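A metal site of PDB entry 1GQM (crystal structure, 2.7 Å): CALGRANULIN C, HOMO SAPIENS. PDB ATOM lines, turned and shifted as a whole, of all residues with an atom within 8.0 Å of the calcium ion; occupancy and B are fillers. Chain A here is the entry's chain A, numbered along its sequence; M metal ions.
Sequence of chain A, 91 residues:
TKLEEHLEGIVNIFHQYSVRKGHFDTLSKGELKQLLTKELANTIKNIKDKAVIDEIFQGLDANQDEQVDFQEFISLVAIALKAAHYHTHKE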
ATOM      1  N   PHE A  14      13.299  28.746  10.280  1.00  0.00           N
ATOM      2  CA  PHE A  14      13.022  27.499   9.615  1.00  0.00           C
ATOM      3  C   PHE A  14      13.128  27.717   8.124  1.00  0.00           C
ATOM      4  O   PHE A  14      13.889  27.025   7.430  1.00  0.00           O
ATOM      5  CB  PHE A  14      11.630  27.029   9.937  1.00  0.00           C
ATOM      6  CG  PHE A  14      11.179  25.886   9.119  1.00  0.00           C
ATOM      7  CD1 PHE A  14      11.675  24.627   9.378  1.00  0.00           C
ATOM      8  CD2 PHE A  14      10.276  26.068   8.076  1.00  0.00           C
ATOM      9  CE1 PHE A  14      11.273  23.548   8.581  1.00  0.00           C
ATOM     10  CE2 PHE A  14       9.861  24.991   7.273  1.00  0.00           C
ATOM     11  CZ  PHE A  14      10.360  23.739   7.509  1.00  0.00           C
ATOM     12  N   HIS A  15      12.381  28.692   7.611  1.00  0.00           N
ATOM     13  CA  HIS A  15      12.341  28.874   6.143  1.00  0.00           C
ATOM     14  C   HIS A  15      13.635  29.293   5.560  1.00  0.00           C
ATOM     15  O   HIS A  15      13.983  28.952   4.431  1.00  0.00           O
ATOM     16  CB  HIS A  15      11.186  29.766   5.706  1.00  0.00           C
ATOM     17  CG  HIS A  15       9.867  29.060   5.757  1.00  0.00           C
ATOM     18  ND1 HIS A  15       8.709  29.658   6.206  1.00  0.00           N
ATOM     19  CD2 HIS A  15       9.543  27.777   5.466  1.00  0.00           C
ATOM     20  CE1 HIS A  15       7.710  28.786   6.169  1.00  0.00           C
ATOM     21  NE2 HIS A  15       8.192  27.640   5.719  1.00  0.00           N
ATOM     22  N   TYR A  17      16.351  28.181   6.260  1.00  0.00           N
ATOM     23  CA  TYR A  17      17.190  27.081   5.921  1.00  0.00           C
ATOM     24  C   TYR A  17      16.490  26.135   4.982  1.00  0.00           C
ATOM     25  O   TYR A  17      17.138  25.382   4.252  1.00  0.00           O
ATOM     26  CB  TYR A  17      17.729  26.388   7.183  1.00  0.00           C
ATOM     27  CG  TYR A  17      18.747  27.227   7.914  1.00  0.00           C
ATOM     28  CD1 TYR A  17      20.086  27.237   7.537  1.00  0.00           C
ATOM     29  CD2 TYR A  17      18.353  28.060   8.934  1.00  0.00           C
ATOM     30  CE1 TYR A  17      21.022  28.045   8.207  1.00  0.00           C
ATOM     31  CE2 TYR A  17      19.267  28.854   9.614  1.00  0.00           C
ATOM     32  CZ  TYR A  17      20.593  28.848   9.244  1.00  0.00           C
ATOM     33  OH  TYR A  17      21.454  29.676   9.936  1.00  0.00           O
ATOM     34  N   SER A  18      15.175  26.151   4.941  1.00  0.00           N
ATOM     35  CA  SER A  18      14.525  25.124   4.113  1.00  0.00           C
ATOM     36  C   SER A  18      14.552  25.383   2.646  1.00  0.00           C
ATOM     37  O   SER A  18      14.516  24.428   1.856  1.00  0.00           O
ATOM     38  CB  SER A  18      13.090  24.782   4.561  1.00  0.00           C
ATOM     39  OG  SER A  18      12.257  25.913   4.742  1.00  0.00           O
ATOM     40  N   VAL A  19      14.635  26.662   2.278  1.00  0.00           N
ATOM     41  CA  VAL A  19      14.665  27.051   0.862  1.00  0.00           C
ATOM     42  C   VAL A  19      15.989  26.866   0.122  1.00  0.00           C
ATOM     43  O   VAL A  19      16.021  27.062  -1.093  1.00  0.00           O
ATOM     44  CB  VAL A  19      14.315  28.551   0.653  1.00  0.00           C
ATOM     45  CG1 VAL A  19      13.197  28.993   1.591  1.00  0.00           C
ATOM     46  CG2 VAL A  19      15.531  29.398   0.888  1.00  0.00           C
ATOM     47  N   ARG A  20      17.087  26.503   0.806  1.00  0.00           N
ATOM     48  CA  ARG A  20      18.356  26.409   0.035  1.00  0.00           C
ATOM     49  C   ARG A  20      18.364  25.298  -1.014  1.00  0.00           C
ATOM     50  O   ARG A  20      18.848  25.502  -2.082  1.00  0.00           O
ATOM     51  CB  ARG A  20      19.615  26.299   0.894  1.00  0.00           C
ATOM     52  CG  ARG A  20      20.053  27.592   1.561  1.00  0.00           C
ATOM     53  CD  ARG A  20      20.432  27.367   3.052  1.00  0.00           C
ATOM     54  NE  ARG A  20      20.286  28.598   3.820  1.00  0.00           N
ATOM     55  CZ  ARG A  20      21.155  29.018   4.736  1.00  0.00           C
ATOM     56  NH1 ARG A  20      22.244  28.286   5.002  1.00  0.00           N
ATOM     57  NH2 ARG A  20      20.923  30.163   5.391  1.00  0.00           N
ATOM     58  N   LYS A  21      17.831  24.125  -0.707  1.00  0.00           N
ATOM     59  CA  LYS A  21      17.793  23.121  -1.725  1.00  0.00           C
ATOM     60  C   LYS A  21      16.589  22.216  -1.569  1.00  0.00           C
ATOM     61  O   LYS A  21      15.965  22.149  -0.494  1.00  0.00           O
ATOM     62  CB  LYS A  21      19.111  22.352  -1.759  1.00  0.00           C
ATOM     63  N   GLY A  22      16.225  21.546  -2.665  1.00  0.00           N
ATOM     64  CA  GLY A  22      15.082  20.651  -2.658  1.00  0.00           C
ATOM     65  C   GLY A  22      13.783  21.367  -2.345  1.00  0.00           C
ATOM     66  O   GLY A  22      13.614  22.533  -2.674  1.00  0.00           O
ATOM     67  N   HIS A  23      12.842  20.665  -1.730  1.00  0.00           N
ATOM     68  CA  HIS A  23      11.572  21.298  -1.452  1.00  0.00           C
ATOM     69  C   HIS A  23      11.825  22.582  -0.612  1.00  0.00           C
ATOM     70  O   HIS A  23      12.744  22.629   0.222  1.00  0.00           O
ATOM     71  CB  HIS A  23      10.600  20.298  -0.795  1.00  0.00           C
ATOM     72  CG  HIS A  23      10.766  18.861  -1.261  1.00  0.00           C
ATOM     73  ND1 HIS A  23      10.240  18.393  -2.442  1.00  0.00           N
ATOM     74  CD2 HIS A  23      11.396  17.807  -0.682  1.00  0.00           C
ATOM     75  CE1 HIS A  23      10.530  17.103  -2.572  1.00  0.00           C
ATOM     76  NE2 HIS A  23      11.239  16.729  -1.513  1.00  0.00           N
ATOM     77  N   PHE A  24      11.056  23.625  -0.865  1.00  0.00           N
ATOM     78  CA  PHE A  24      11.242  24.907  -0.171  1.00  0.00           C
ATOM     79  C   PHE A  24      10.708  24.743   1.216  1.00  0.00           C
ATOM     80  O   PHE A  24      11.155  25.376   2.166  1.00  0.00           O
ATOM     81  CB  PHE A  24      10.418  26.034  -0.851  1.00  0.00           C
ATOM     82  CG  PHE A  24      11.077  26.652  -2.094  1.00  0.00           C
ATOM     83  CD1 PHE A  24      12.371  26.330  -2.488  1.00  0.00           C
ATOM     84  CD2 PHE A  24      10.378  27.574  -2.870  1.00  0.00           C
ATOM     85  CE1 PHE A  24      12.959  26.903  -3.633  1.00  0.00           C
ATOM     86  CE2 PHE A  24      10.949  28.150  -4.029  1.00  0.00           C
ATOM     87  CZ  PHE A  24      12.249  27.818  -4.404  1.00  0.00           C
ATOM     88  N   ASP A  25       9.731  23.851   1.313  1.00  0.00           N
ATOM     89  CA  ASP A  25       8.934  23.713   2.501  1.00  0.00           C
ATOM     90  C   ASP A  25       9.534  22.783   3.542  1.00  0.00           C
ATOM     91  O   ASP A  25       8.986  22.629   4.638  1.00  0.00           O
ATOM     92  CB  ASP A  25       7.495  23.329   2.084  1.00  0.00           C
ATOM     93  CG  ASP A  25       7.438  22.358   0.876  1.00  0.00           C
ATOM     94  OD1 ASP A  25       6.722  22.626  -0.133  1.00  0.00           O
ATOM     95  OD2 ASP A  25       8.077  21.278   0.836  1.00  0.00           O
ATOM     96  N   THR A  26      10.655  22.159   3.231  1.00  0.00           N
ATOM     97  CA  THR A  26      11.239  21.189   4.159  1.00  0.00           C
ATOM     98  C   THR A  26      12.752  21.307   4.229  1.00  0.00           C
ATOM     99  O   THR A  26      13.372  21.990   3.364  1.00  0.00           O
ATOM    100  CB  THR A  26      10.846  19.753   3.760  1.00  0.00           C
ATOM    101  OG1 THR A  26      11.119  19.541   2.355  1.00  0.00           O
ATOM    102  CG2 THR A  26       9.316  19.597   3.852  1.00  0.00           C
ATOM    103  N   LEU A  27      13.331  20.668   5.241  1.00  0.00           N
ATOM    104  CA  LEU A  27      14.755  20.689   5.528  1.00  0.00           C
ATOM    105  C   LEU A  27      15.408  19.356   5.224  1.00  0.00           C
ATOM    106  O   LEU A  27      15.011  18.313   5.752  1.00  0.00           O
ATOM    107  CB  LEU A  27      14.972  20.934   7.018  1.00  0.00           C
ATOM    108  CG  LEU A  27      14.590  22.305   7.550  1.00  0.00           C
ATOM    109  CD1 LEU A  27      14.298  22.242   9.034  1.00  0.00           C
ATOM    110  CD2 LEU A  27      15.714  23.320   7.220  1.00  0.00           C
ATOM    111  N   SER A  28      16.448  19.383   4.422  1.00  0.00           N
ATOM    112  CA  SER A  28      17.147  18.153   4.106  1.00  0.00           C
ATOM    113  C   SER A  28      18.109  17.863   5.223  1.00  0.00           C
ATOM    114  O   SER A  28      18.354  18.734   6.052  1.00  0.00           O
ATOM    115  CB  SER A  28      17.978  18.390   2.857  1.00  0.00           C
ATOM    116  OG  SER A  28      18.919  19.400   3.158  1.00  0.00           O
ATOM    117  N   LYS A  29      18.704  16.671   5.206  1.00  0.00           N
ATOM    118  CA  LYS A  29      19.731  16.391   6.184  1.00  0.00           C
ATOM    119  C   LYS A  29      20.709  17.573   6.180  1.00  0.00           C
ATOM    120  O   LYS A  29      20.989  18.162   7.217  1.00  0.00           O
ATOM    121  CB  LYS A  29      20.463  15.083   5.887  1.00  0.00           C
ATOM    122  CG  LYS A  29      21.058  14.483   7.165  1.00  0.00           C
ATOM    123  CD  LYS A  29      20.981  12.972   7.162  1.00  0.00           C
ATOM    124  N   GLU A  31      20.406  20.656   4.976  1.00  0.00           N
ATOM    125  CA  GLU A  31      19.832  21.906   5.433  1.00  0.00           C
ATOM    126  C   GLU A  31      19.762  21.902   6.970  1.00  0.00           C
ATOM    127  O   GLU A  31      20.085  22.899   7.617  1.00  0.00           O
ATOM    128  CB  GLU A  31      18.442  22.108   4.830  1.00  0.00           C
ATOM    129  CG  GLU A  31      18.479  22.706   3.451  1.00  0.00           C
ATOM    130  CD  GLU A  31      17.149  22.632   2.727  1.00  0.00           C
ATOM    131  OE1 GLU A  31      16.374  21.668   2.942  1.00  0.00           O
ATOM    132  OE2 GLU A  31      16.894  23.526   1.871  1.00  0.00           O
ATOM    133  N   LEU A  32      19.392  20.762   7.520  1.00  0.00           N
ATOM    134  CA  LEU A  32      19.233  20.662   8.945  1.00  0.00           C
ATOM    135  C   LEU A  32      20.554  20.783   9.695  1.00  0.00           C
ATOM    136  O   LEU A  32      20.614  21.346  10.788  1.00  0.00           O
ATOM    137  CB  LEU A  32      18.539  19.378   9.316  1.00  0.00           C
ATOM    138  CG  LEU A  32      18.339  19.214  10.816  1.00  0.00           C
ATOM    139  CD1 LEU A  32      17.499  20.334  11.318  1.00  0.00           C
ATOM    140  CD2 LEU A  32      17.706  17.914  11.082  1.00  0.00           C
ATOM    141  N   GLN A  67      13.151  13.876   5.106  1.00  0.00           N
ATOM    142  CA  GLN A  67      13.010  15.317   5.221  1.00  0.00           C
ATOM    143  C   GLN A  67      12.459  15.710   6.573  1.00  0.00           C
ATOM    144  O   GLN A  67      11.809  14.910   7.267  1.00  0.00           O
ATOM    145  CB  GLN A  67      12.149  15.927   4.128  1.00  0.00           C
ATOM    146  CG  GLN A  67      12.602  15.649   2.688  1.00  0.00           C
ATOM    147  CD  GLN A  67      13.710  16.574   2.179  1.00  0.00           C
ATOM    148  OE1 GLN A  67      13.679  17.776   2.413  1.00  0.00           O
ATOM    149  NE2 GLN A  67      14.666  16.010   1.460  1.00  0.00           N
ATOM    150  N   VAL A  68      12.723  16.937   6.969  1.00  0.00           N
ATOM    151  CA  VAL A  68      12.175  17.380   8.219  1.00  0.00           C
ATOM    152  C   VAL A  68      11.245  18.479   7.874  1.00  0.00           C
ATOM    153  O   VAL A  68      11.709  19.520   7.447  1.00  0.00           O
ATOM    154  CB  VAL A  68      13.236  17.899   9.123  1.00  0.00           C
ATOM    155  CG1 VAL A  68      12.606  18.643  10.329  1.00  0.00           C
ATOM    156  CG2 VAL A  68      14.060  16.748   9.616  1.00  0.00           C
HETATM  157 CA    CA M   1      14.773  21.966   1.456  1.00  0.00          CA
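OE1 of Glu 31 binds the calcium ion, 2.2 Å away. O of Lys 21 is bound to the calcium ion (2.3 Å). O of Thr 26 binds the calcium ion. The backbone carbonyl oxygen (O) of His 23 is bound to the calcium ion (2.5 Å). O of Ser 18 binds the calcium ion. The calcium ion is bound by OE2 of Glu 31 (2.7 Å).
Merely in contact with the calcium ion: Gly 22. Of the 19 residues printed, 6 come within 4 Å of the calcium ion. The nearest printed residue that does not touch the calcium ion is Leu 27 (4.3 Å).
The side-chain hydroxyl of Ser 28 lies within hydrogen-bond range of the backbone NH of Glu 31 (2.7 Å). The side-chain carboxylate (OE2) of Glu 31 sits close to the backbone NH (N) of Arg 20 (3.2 Å). OG1 of Thr 26 sits at hydrogen-bond distance from OE1 of Gln 67, 3.1 Å away. O of Phe 24 lies within hydrogen-bond range of OG of Ser 18, 2.9 Å away. The side-chain hydroxyl (OG) of Ser 18 lies within hydrogen-bond range of the backbone carbonyl oxygen (O) of Phe 14.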
